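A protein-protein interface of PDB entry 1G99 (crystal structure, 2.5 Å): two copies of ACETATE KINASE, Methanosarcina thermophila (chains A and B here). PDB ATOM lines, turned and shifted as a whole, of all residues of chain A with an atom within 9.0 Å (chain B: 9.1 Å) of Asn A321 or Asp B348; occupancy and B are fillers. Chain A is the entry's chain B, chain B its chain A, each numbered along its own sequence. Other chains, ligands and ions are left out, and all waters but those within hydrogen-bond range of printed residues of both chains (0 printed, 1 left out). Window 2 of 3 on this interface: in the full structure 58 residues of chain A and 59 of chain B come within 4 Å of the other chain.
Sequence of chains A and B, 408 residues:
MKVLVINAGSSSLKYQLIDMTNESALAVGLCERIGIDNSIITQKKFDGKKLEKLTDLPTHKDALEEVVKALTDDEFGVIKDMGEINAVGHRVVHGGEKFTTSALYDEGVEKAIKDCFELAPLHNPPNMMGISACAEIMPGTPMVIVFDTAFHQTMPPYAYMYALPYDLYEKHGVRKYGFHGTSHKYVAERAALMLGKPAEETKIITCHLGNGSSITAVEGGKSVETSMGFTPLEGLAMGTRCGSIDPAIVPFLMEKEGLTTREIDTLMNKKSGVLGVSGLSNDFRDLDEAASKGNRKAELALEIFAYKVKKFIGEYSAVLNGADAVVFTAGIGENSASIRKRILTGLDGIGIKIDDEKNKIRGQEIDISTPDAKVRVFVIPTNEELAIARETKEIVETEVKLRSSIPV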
ATOM      1  N   LYS A 203     -11.780  12.774  10.051  1.00  0.00           N
ATOM      2  CA  LYS A 203     -10.628  13.560  10.476  1.00  0.00           C
ATOM      3  C   LYS A 203     -11.215  14.944  10.759  1.00  0.00           C
ATOM      4  O   LYS A 203     -11.661  15.647   9.854  1.00  0.00           O
ATOM      5  CB  LYS A 203      -9.532  13.584   9.396  1.00  0.00           C
ATOM      6  CG  LYS A 203      -9.033  12.172   9.064  1.00  0.00           C
ATOM      7  CD  LYS A 203      -7.625  12.181   8.554  1.00  0.00           C
ATOM      8  CE  LYS A 203      -7.543  11.882   7.071  1.00  0.00           C
ATOM      9  NZ  LYS A 203      -8.293  12.851   6.252  1.00  0.00           N
ATOM     10  N   ILE A 205     -11.017  18.770  13.087  1.00  0.00           N
ATOM     11  CA  ILE A 205     -10.240  19.733  13.877  1.00  0.00           C
ATOM     12  C   ILE A 205     -11.291  20.420  14.756  1.00  0.00           C
ATOM     13  O   ILE A 205     -12.260  20.999  14.236  1.00  0.00           O
ATOM     14  CB  ILE A 205      -9.551  20.781  12.989  1.00  0.00           C
ATOM     15  CG1 ILE A 205      -8.493  20.101  12.119  1.00  0.00           C
ATOM     16  CG2 ILE A 205      -8.976  21.894  13.851  1.00  0.00           C
ATOM     17  CD1 ILE A 205      -7.907  21.015  11.092  1.00  0.00           C
ATOM     18  N   ALA A 217      -6.724  17.966  17.155  1.00  0.00           N
ATOM     19  CA  ALA A 217      -6.749  17.241  15.889  1.00  0.00           C
ATOM     20  C   ALA A 217      -7.290  15.865  16.249  1.00  0.00           C
ATOM     21  O   ALA A 217      -6.642  15.108  16.966  1.00  0.00           O
ATOM     22  CB  ALA A 217      -5.364  17.130  15.335  1.00  0.00           C
ATOM     23  N   GLU A 219      -8.390  12.260  14.991  1.00  0.00           N
ATOM     24  CA  GLU A 219      -8.288  11.289  13.922  1.00  0.00           C
ATOM     25  C   GLU A 219      -9.009   9.999  14.224  1.00  0.00           C
ATOM     26  O   GLU A 219      -8.605   9.273  15.119  1.00  0.00           O
ATOM     27  CB  GLU A 219      -6.841  10.976  13.668  1.00  0.00           C
ATOM     28  CG  GLU A 219      -6.661  10.066  12.520  1.00  0.00           C
ATOM     29  CD  GLU A 219      -5.227   9.991  12.133  1.00  0.00           C
ATOM     30  OE1 GLU A 219      -4.436   9.488  12.959  1.00  0.00           O
ATOM     31  OE2 GLU A 219      -4.891  10.450  11.015  1.00  0.00           O
ATOM     32  N   VAL A 224      -5.107  13.265  18.676  1.00  0.00           N
ATOM     33  CA  VAL A 224      -3.792  12.947  18.204  1.00  0.00           C
ATOM     34  C   VAL A 224      -2.803  14.087  18.409  1.00  0.00           C
ATOM     35  O   VAL A 224      -1.589  13.884  18.301  1.00  0.00           O
ATOM     36  CB  VAL A 224      -3.939  12.527  16.701  1.00  0.00           C
ATOM     37  CG1 VAL A 224      -2.999  13.243  15.850  1.00  0.00           C
ATOM     38  CG2 VAL A 224      -3.822  11.016  16.578  1.00  0.00           C
ATOM     39  N   ILE A 313      -5.409  25.878  12.336  1.00  0.00           N
ATOM     40  CA  ILE A 313      -6.184  25.109  11.393  1.00  0.00           C
ATOM     41  C   ILE A 313      -5.206  24.611  10.318  1.00  0.00           C
ATOM     42  O   ILE A 313      -5.294  23.464   9.870  1.00  0.00           O
ATOM     43  CB  ILE A 313      -7.301  25.973  10.799  1.00  0.00           C
ATOM     44  CG1 ILE A 313      -8.331  26.287  11.900  1.00  0.00           C
ATOM     45  CG2 ILE A 313      -7.960  25.247   9.599  1.00  0.00           C
ATOM     46  CD1 ILE A 313      -9.453  27.235  11.470  1.00  0.00           C
ATOM     47  N   GLY A 314      -4.249  25.452   9.923  1.00  0.00           N
ATOM     48  CA  GLY A 314      -3.287  25.028   8.925  1.00  0.00           C
ATOM     49  C   GLY A 314      -2.428  23.909   9.508  1.00  0.00           C
ATOM     50  O   GLY A 314      -2.209  22.857   8.886  1.00  0.00           O
ATOM     51  N   GLU A 315      -1.952  24.135  10.726  1.00  0.00           N
ATOM     52  CA  GLU A 315      -1.086  23.193  11.428  1.00  0.00           C
ATOM     53  C   GLU A 315      -1.699  21.793  11.562  1.00  0.00           C
ATOM     54  O   GLU A 315      -1.067  20.776  11.226  1.00  0.00           O
ATOM     55  CB  GLU A 315      -0.718  23.746  12.821  1.00  0.00           C
ATOM     56  CG  GLU A 315       0.324  22.930  13.561  1.00  0.00           C
ATOM     57  CD  GLU A 315       0.630  23.496  14.927  1.00  0.00           C
ATOM     58  OE1 GLU A 315       0.663  24.729  15.060  1.00  0.00           O
ATOM     59  OE2 GLU A 315       0.847  22.724  15.873  1.00  0.00           O
ATOM     60  N   TYR A 316      -2.934  21.733  12.026  1.00  0.00           N
ATOM     61  CA  TYR A 316      -3.595  20.440  12.173  1.00  0.00           C
ATOM     62  C   TYR A 316      -4.070  19.832  10.843  1.00  0.00           C
ATOM     63  O   TYR A 316      -4.365  18.645  10.780  1.00  0.00           O
ATOM     64  CB  TYR A 316      -4.714  20.547  13.204  1.00  0.00           C
ATOM     65  CG  TYR A 316      -4.155  20.803  14.580  1.00  0.00           C
ATOM     66  CD1 TYR A 316      -2.769  20.959  14.777  1.00  0.00           C
ATOM     67  CD2 TYR A 316      -4.992  20.901  15.688  1.00  0.00           C
ATOM     68  CE1 TYR A 316      -2.239  21.212  16.036  1.00  0.00           C
ATOM     69  CE2 TYR A 316      -4.483  21.145  16.954  1.00  0.00           C
ATOM     70  CZ  TYR A 316      -3.114  21.301  17.127  1.00  0.00           C
ATOM     71  OH  TYR A 316      -2.621  21.524  18.392  1.00  0.00           O
ATOM     72  N   SER A 317      -4.116  20.637   9.780  1.00  0.00           N
ATOM     73  CA  SER A 317      -4.457  20.102   8.458  1.00  0.00           C
ATOM     74  C   SER A 317      -3.259  19.250   8.022  1.00  0.00           C
ATOM     75  O   SER A 317      -3.430  18.225   7.367  1.00  0.00           O
ATOM     76  CB  SER A 317      -4.700  21.224   7.430  1.00  0.00           C
ATOM     77  OG  SER A 317      -5.994  21.774   7.594  1.00  0.00           O
ATOM     78  N   ALA A 318      -2.040  19.669   8.381  1.00  0.00           N
ATOM     79  CA  ALA A 318      -0.857  18.864   8.040  1.00  0.00           C
ATOM     80  C   ALA A 318      -0.808  17.625   8.951  1.00  0.00           C
ATOM     81  O   ALA A 318      -0.492  16.546   8.496  1.00  0.00           O
ATOM     82  CB  ALA A 318       0.426  19.664   8.209  1.00  0.00           C
ATOM     83  N   VAL A 319      -1.116  17.792  10.242  1.00  0.00           N
ATOM     84  CA  VAL A 319      -1.086  16.687  11.179  1.00  0.00           C
ATOM     85  C   VAL A 319      -2.028  15.581  10.710  1.00  0.00           C
ATOM     86  O   VAL A 319      -1.653  14.423  10.640  1.00  0.00           O
ATOM     87  CB  VAL A 319      -1.509  17.147  12.570  1.00  0.00           C
ATOM     88  CG1 VAL A 319      -1.803  15.919  13.493  1.00  0.00           C
ATOM     89  CG2 VAL A 319      -0.420  17.997  13.159  1.00  0.00           C
ATOM     90  N   LEU A 320      -3.247  15.958  10.357  1.00  0.00           N
ATOM     91  CA  LEU A 320      -4.258  15.021   9.894  1.00  0.00           C
ATOM     92  C   LEU A 320      -4.177  14.617   8.420  1.00  0.00           C
ATOM     93  O   LEU A 320      -4.922  13.743   8.000  1.00  0.00           O
ATOM     94  CB  LEU A 320      -5.642  15.622  10.135  1.00  0.00           C
ATOM     95  CG  LEU A 320      -6.008  15.868  11.590  1.00  0.00           C
ATOM     96  CD1 LEU A 320      -7.337  16.603  11.691  1.00  0.00           C
ATOM     97  CD2 LEU A 320      -6.060  14.531  12.279  1.00  0.00           C
ATOM     98  N   ASN A 321      -3.276  15.236   7.649  1.00  0.00           N
ATOM     99  CA  ASN A 321      -3.169  14.972   6.212  1.00  0.00           C
ATOM    100  C   ASN A 321      -4.494  15.305   5.485  1.00  0.00           C
ATOM    101  O   ASN A 321      -4.999  14.515   4.705  1.00  0.00           O
ATOM    102  CB  ASN A 321      -2.816  13.512   5.923  1.00  0.00           C
ATOM    103  CG  ASN A 321      -2.311  13.321   4.485  1.00  0.00           C
ATOM    104  OD1 ASN A 321      -2.110  14.294   3.741  1.00  0.00           O
ATOM    105  ND2 ASN A 321      -2.104  12.079   4.094  1.00  0.00           N
ATOM    106  N   GLY A 322      -5.027  16.494   5.735  1.00  0.00           N
ATOM    107  CA  GLY A 322      -6.288  16.899   5.141  1.00  0.00           C
ATOM    108  C   GLY A 322      -7.404  16.574   6.133  1.00  0.00           C
ATOM    109  O   GLY A 322      -7.560  15.428   6.534  1.00  0.00           O
ATOM    110  N   ALA A 323      -8.170  17.569   6.551  1.00  0.00           N
ATOM    111  CA  ALA A 323      -9.246  17.337   7.496  1.00  0.00           C
ATOM    112  C   ALA A 323     -10.600  17.283   6.763  1.00  0.00           C
ATOM    113  O   ALA A 323     -10.744  17.871   5.686  1.00  0.00           O
ATOM    114  CB  ALA A 323      -9.251  18.470   8.537  1.00  0.00           C
ATOM    115  N   ASP A 324     -11.589  16.586   7.332  1.00  0.00           N
ATOM    116  CA  ASP A 324     -12.910  16.527   6.715  1.00  0.00           C
ATOM    117  C   ASP A 324     -13.741  17.720   7.207  1.00  0.00           C
ATOM    118  O   ASP A 324     -14.583  18.250   6.477  1.00  0.00           O
ATOM    119  CB  ASP A 324     -13.651  15.242   7.090  1.00  0.00           C
ATOM    120  CG  ASP A 324     -12.891  13.995   6.680  1.00  0.00           C
ATOM    121  OD1 ASP A 324     -12.389  13.969   5.532  1.00  0.00           O
ATOM    122  OD2 ASP A 324     -12.793  13.041   7.500  1.00  0.00           O
ATOM    123  N   LYS A 374     -14.486  21.885   0.159  1.00  0.00           N
ATOM    124  CA  LYS A 374     -13.985  20.544   0.404  1.00  0.00           C
ATOM    125  C   LYS A 374     -14.055  20.218   1.905  1.00  0.00           C
ATOM    126  O   LYS A 374     -14.406  19.103   2.308  1.00  0.00           O
ATOM    127  CB  LYS A 374     -12.553  20.451  -0.124  1.00  0.00           C
ATOM    128  CG  LYS A 374     -11.894  19.098   0.048  1.00  0.00           C
ATOM    129  CD  LYS A 374     -10.495  19.083  -0.580  1.00  0.00           C
ATOM    130  CE  LYS A 374      -9.875  17.677  -0.578  1.00  0.00           C
ATOM    131  NZ  LYS A 374     -10.643  16.667  -1.380  1.00  0.00           N
ATOM    132  N   LYS B 310       6.970  19.509   9.714  1.00  0.00           N
ATOM    133  CA  LYS B 310       5.748  19.165   9.004  1.00  0.00           C
ATOM    134  C   LYS B 310       4.598  20.081   9.442  1.00  0.00           C
ATOM    135  O   LYS B 310       3.852  20.605   8.604  1.00  0.00           O
ATOM    136  CB  LYS B 310       5.462  17.692   9.267  1.00  0.00           C
ATOM    137  CG  LYS B 310       4.115  17.162   8.864  1.00  0.00           C
ATOM    138  CD  LYS B 310       4.263  15.656   8.783  1.00  0.00           C
ATOM    139  CE  LYS B 310       2.955  14.993   8.847  1.00  0.00           C
ATOM    140  NZ  LYS B 310       3.152  13.541   8.638  1.00  0.00           N
ATOM    141  N   GLY B 314       2.111  23.054   7.500  1.00  0.00           N
ATOM    142  CA  GLY B 314       0.660  23.206   7.538  1.00  0.00           C
ATOM    143  C   GLY B 314       0.285  24.631   7.984  1.00  0.00           C
ATOM    144  O   GLY B 314      -0.556  25.298   7.389  1.00  0.00           O
ATOM    145  N   ILE B 343       9.892  14.264   6.963  1.00  0.00           N
ATOM    146  CA  ILE B 343       9.085  15.475   6.989  1.00  0.00           C
ATOM    147  C   ILE B 343       7.937  15.467   5.988  1.00  0.00           C
ATOM    148  O   ILE B 343       6.822  15.835   6.324  1.00  0.00           O
ATOM    149  CB  ILE B 343       9.960  16.703   6.687  1.00  0.00           C
ATOM    150  CG1 ILE B 343      10.980  16.887   7.807  1.00  0.00           C
ATOM    151  CG2 ILE B 343       9.077  17.937   6.406  1.00  0.00           C
ATOM    152  CD1 ILE B 343      12.032  17.879   7.464  1.00  0.00           C
ATOM    153  N   LEU B 344       8.215  15.034   4.762  1.00  0.00           N
ATOM    154  CA  LEU B 344       7.231  15.093   3.700  1.00  0.00           C
ATOM    155  C   LEU B 344       6.263  13.937   3.531  1.00  0.00           C
ATOM    156  O   LEU B 344       5.443  13.944   2.623  1.00  0.00           O
ATOM    157  CB  LEU B 344       7.969  15.370   2.383  1.00  0.00           C
ATOM    158  CG  LEU B 344       8.740  16.686   2.389  1.00  0.00           C
ATOM    159  CD1 LEU B 344       9.797  16.689   1.303  1.00  0.00           C
ATOM    160  CD2 LEU B 344       7.723  17.849   2.199  1.00  0.00           C
ATOM    161  N   THR B 345       6.342  12.944   4.394  1.00  0.00           N
ATOM    162  CA  THR B 345       5.435  11.807   4.317  1.00  0.00           C
ATOM    163  C   THR B 345       4.085  12.180   4.931  1.00  0.00           C
ATOM    164  O   THR B 345       4.040  12.850   5.946  1.00  0.00           O
ATOM    165  CB  THR B 345       6.006  10.612   5.087  1.00  0.00           C
ATOM    166  OG1 THR B 345       7.208  10.176   4.443  1.00  0.00           O
ATOM    167  CG2 THR B 345       5.008   9.477   5.109  1.00  0.00           C
ATOM    168  N   GLY B 346       2.994  11.756   4.306  1.00  0.00           N
ATOM    169  CA  GLY B 346       1.669  12.053   4.825  1.00  0.00           C
ATOM    170  C   GLY B 346       1.132  13.453   4.589  1.00  0.00           C
ATOM    171  O   GLY B 346       0.394  13.970   5.418  1.00  0.00           O
ATOM    172  N   LEU B 347       1.506  14.097   3.484  1.00  0.00           N
ATOM    173  CA  LEU B 347       1.000  15.454   3.209  1.00  0.00           C
ATOM    174  C   LEU B 347       0.294  15.553   1.855  1.00  0.00           C
ATOM    175  O   LEU B 347      -0.016  16.650   1.383  1.00  0.00           O
ATOM    176  CB  LEU B 347       2.144  16.485   3.279  1.00  0.00           C
ATOM    177  CG  LEU B 347       2.720  16.715   4.684  1.00  0.00           C
ATOM    178  CD1 LEU B 347       3.913  17.649   4.648  1.00  0.00           C
ATOM    179  CD2 LEU B 347       1.617  17.272   5.578  1.00  0.00           C
ATOM    180  N   ASP B 348       0.019  14.410   1.232  1.00  0.00           N
ATOM    181  CA  ASP B 348      -0.637  14.422  -0.074  1.00  0.00           C
ATOM    182  C   ASP B 348      -1.986  15.086   0.099  1.00  0.00           C
ATOM    183  O   ASP B 348      -2.496  15.744  -0.811  1.00  0.00           O
ATOM    184  CB  ASP B 348      -0.791  13.002  -0.634  1.00  0.00           C
ATOM    185  CG  ASP B 348      -1.458  12.056   0.344  1.00  0.00           C
ATOM    186  OD1 ASP B 348      -0.821  11.684   1.339  1.00  0.00           O
ATOM    187  OD2 ASP B 348      -2.624  11.688   0.125  1.00  0.00           O
ATOM    188  N   GLY B 349      -2.536  14.952   1.300  1.00  0.00           N
ATOM    189  CA  GLY B 349      -3.817  15.564   1.589  1.00  0.00           C
ATOM    190  C   GLY B 349      -3.817  17.073   1.406  1.00  0.00           C
ATOM    191  O   GLY B 349      -4.889  17.682   1.287  1.00  0.00           O
ATOM    192  N   ILE B 350      -2.645  17.703   1.425  1.00  0.00           N
ATOM    193  CA  ILE B 350      -2.604  19.138   1.198  1.00  0.00           C
ATOM    194  C   ILE B 350      -1.779  19.467  -0.063  1.00  0.00           C
ATOM    195  O   ILE B 350      -1.158  20.521  -0.178  1.00  0.00           O
ATOM    196  CB  ILE B 350      -2.073  19.918   2.440  1.00  0.00           C
ATOM    197  CG1 ILE B 350      -0.704  19.419   2.871  1.00  0.00           C
ATOM    198  CG2 ILE B 350      -3.028  19.760   3.605  1.00  0.00           C
ATOM    199  CD1 ILE B 350      -0.086  20.316   3.904  1.00  0.00           C
ATOM    200  N   GLY B 351      -1.765  18.536  -1.015  1.00  0.00           N
ATOM    201  CA  GLY B 351      -1.057  18.788  -2.253  1.00  0.00           C
ATOM    202  C   GLY B 351       0.423  18.501  -2.347  1.00  0.00           C
ATOM    203  O   GLY B 351       1.047  18.826  -3.354  1.00  0.00           O
ATOM    204  N   ILE B 352       0.999  17.893  -1.324  1.00  0.00           N
ATOM    205  CA  ILE B 352       2.422  17.609  -1.347  1.00  0.00           C
ATOM    206  C   ILE B 352       2.733  16.108  -1.512  1.00  0.00           C
ATOM    207  O   ILE B 352       2.342  15.272  -0.691  1.00  0.00           O
ATOM    208  CB  ILE B 352       3.073  18.149  -0.069  1.00  0.00           C
ATOM    209  CG1 ILE B 352       2.968  19.670  -0.059  1.00  0.00           C
ATOM    210  CG2 ILE B 352       4.532  17.710   0.016  1.00  0.00           C
ATOM    211  CD1 ILE B 352       3.537  20.313   1.202  1.00  0.00           C
ATOM    212  N   LYS B 353       3.443  15.781  -2.587  1.00  0.00           N
ATOM    213  CA  LYS B 353       3.813  14.400  -2.862  1.00  0.00           C
ATOM    214  C   LYS B 353       5.204  14.413  -3.510  1.00  0.00           C
ATOM    215  O   LYS B 353       5.443  15.153  -4.461  1.00  0.00           O
ATOM    216  CB  LYS B 353       2.785  13.803  -3.806  1.00  0.00           C
ATOM    217  CG  LYS B 353       2.588  12.313  -3.672  1.00  0.00           C
ATOM    218  CD  LYS B 353       1.827  11.760  -4.883  1.00  0.00           C
ATOM    219  CE  LYS B 353       0.567  12.569  -5.206  1.00  0.00           C
ATOM    220  NZ  LYS B 353      -0.026  12.119  -6.501  1.00  0.00           N
ATOM    221  N   ILE B 354       6.129  13.614  -3.002  1.00  0.00           N
ATOM    222  CA  ILE B 354       7.458  13.621  -3.573  1.00  0.00           C
ATOM    223  C   ILE B 354       7.842  12.315  -4.219  1.00  0.00           C
ATOM    224  O   ILE B 354       7.220  11.284  -3.977  1.00  0.00           O
ATOM    225  CB  ILE B 354       8.542  13.931  -2.521  1.00  0.00           C
ATOM    226  CG1 ILE B 354       8.579  12.814  -1.499  1.00  0.00           C
ATOM    227  CG2 ILE B 354       8.317  15.329  -1.910  1.00  0.00           C
ATOM    228  CD1 ILE B 354       9.879  12.795  -0.735  1.00  0.00           C
ATOM    229  N   THR B 370       6.371  14.887  -7.352  1.00  0.00           N
ATOM    230  CA  THR B 370       5.839  14.150  -8.482  1.00  0.00           C
ATOM    231  C   THR B 370       5.271  15.224  -9.421  1.00  0.00           C
ATOM    232  O   THR B 370       4.864  16.298  -8.989  1.00  0.00           O
ATOM    233  CB  THR B 370       4.735  13.179  -8.032  1.00  0.00           C
ATOM    234  OG1 THR B 370       3.695  13.909  -7.382  1.00  0.00           O
ATOM    235  CG2 THR B 370       5.298  12.151  -7.050  1.00  0.00           C
ATOM    236  N   ASP B 372       2.475  15.531 -10.820  1.00  0.00           N
ATOM    237  CA  ASP B 372       1.053  15.849 -10.622  1.00  0.00           C
ATOM    238  C   ASP B 372       0.754  16.566  -9.286  1.00  0.00           C
ATOM    239  O   ASP B 372      -0.369  16.992  -9.076  1.00  0.00           O
ATOM    240  CB  ASP B 372       0.200  14.556 -10.704  1.00  0.00           C
ATOM    241  CG  ASP B 372       0.533  13.567  -9.602  1.00  0.00           C
ATOM    242  OD1 ASP B 372       1.733  13.312  -9.364  1.00  0.00           O
ATOM    243  OD2 ASP B 372      -0.402  13.049  -8.959  1.00  0.00           O
ATOM    244  N   ALA B 373       1.731  16.673  -8.386  1.00  0.00           N
ATOM    245  CA  ALA B 373       1.502  17.327  -7.079  1.00  0.00           C
ATOM    246  C   ALA B 373       1.133  18.795  -7.275  1.00  0.00           C
ATOM    247  O   ALA B 373       1.715  19.471  -8.111  1.00  0.00           O
ATOM    248  CB  ALA B 373       2.749  17.206  -6.194  1.00  0.00           C
ATOM    249  N   LYS B 374       0.129  19.266  -6.536  1.00  0.00           N
ATOM    250  CA  LYS B 374      -0.300  20.654  -6.615  1.00  0.00           C
ATOM    251  C   LYS B 374       0.803  21.602  -6.098  1.00  0.00           C
ATOM    252  O   LYS B 374       0.993  22.654  -6.666  1.00  0.00           O
ATOM    253  CB  LYS B 374      -1.604  20.865  -5.822  1.00  0.00           C
ATOM    254  N   VAL B 375       1.548  21.214  -5.056  1.00  0.00           N
ATOM    255  CA  VAL B 375       2.612  22.038  -4.465  1.00  0.00           C
ATOM    256  C   VAL B 375       3.979  21.493  -4.865  1.00  0.00           C
ATOM    257  O   VAL B 375       4.241  20.300  -4.718  1.00  0.00           O
ATOM    258  CB  VAL B 375       2.525  22.007  -2.901  1.00  0.00           C
ATOM    259  CG1 VAL B 375       3.573  22.932  -2.278  1.00  0.00           C
ATOM    260  CG2 VAL B 375       1.094  22.393  -2.445  1.00  0.00           C
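The side-chain carboxylate (OD1) of Asp B348 is in hydrogen-bond range of the side-chain amide nitrogen (ND2) of Asn A321 (3.1 Å).
O of Gly B346 sits close to OD1 of Asn A321, 3.0 Å away.
The backbone carbonyl oxygen (O) of Gly A314 lies close to the backbone carbonyl oxygen (O) of Gly B314, at 3.3 Å.
OD1 of Asn A321 sits at hydrogen-bond distance from N of Gly B349 (2.6 Å).
The side-chain amino group (NZ) of Lys B310 lies within hydrogen-bond range of the backbone carbonyl oxygen (O) of Thr B345 (2.9 Å).
The backbone carbonyl oxygen (O) of Leu B347 lies within hydrogen-bond range of the backbone NH (N) of Ile B352 (3.1 Å).
Among the printed residues, pairs that only touch across the chains: Asn A321 with Leu B347, Glu A315 with Gly B314, Ala A318 with Lys B310, Ala A318 with Gly B314 and Ala A318 with Leu B347.
Of chain B, only Gly B346 (2.9 Å), Leu B347 (3.3 Å), Asp B348 (3.1 Å) and Gly B349 (2.6 Å) come within 4 Å of Asn A321.
No residue of chain B comes within 4 Å of Gly A322.
Gly B346 touches one residue of chain A.
Printed residues of chain A within 4 Å of Gly B314: Gly A314, Glu A315 and Ala A318.
Of the printed residues of chain B, Glu A315 touches Gly B314 (3.6 Å).
Of the printed residues of chain B, Ala A318 touches Lys B310, Gly B314 and Leu B347.
Lys A374 touches none of the printed residues of chain B.
Lys B353 touches none of the printed residues of chain A.
The nearest residue of chain B that does not touch Asn A321 is Ile B350 (4.2 Å).
Of the 18 printed residues of chain A, 4 touch a printed residue of chain B.
Hydrophobic or aromatic side chains of chain A that line the printed part of chain B: Ala A318.
Of the 19 printed residues of chain B, 6 touch a printed residue of chain A.
Hydrophobic or aromatic side chains of chain B that line the printed part of chain A: Leu B347.
Among the printed residues, no Asp or Glu carboxylate lies within 4 Å of a Lys or Arg side-chain nitrogen of the other chain.
Gly A314 touches its own counterpart, Gly B314.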
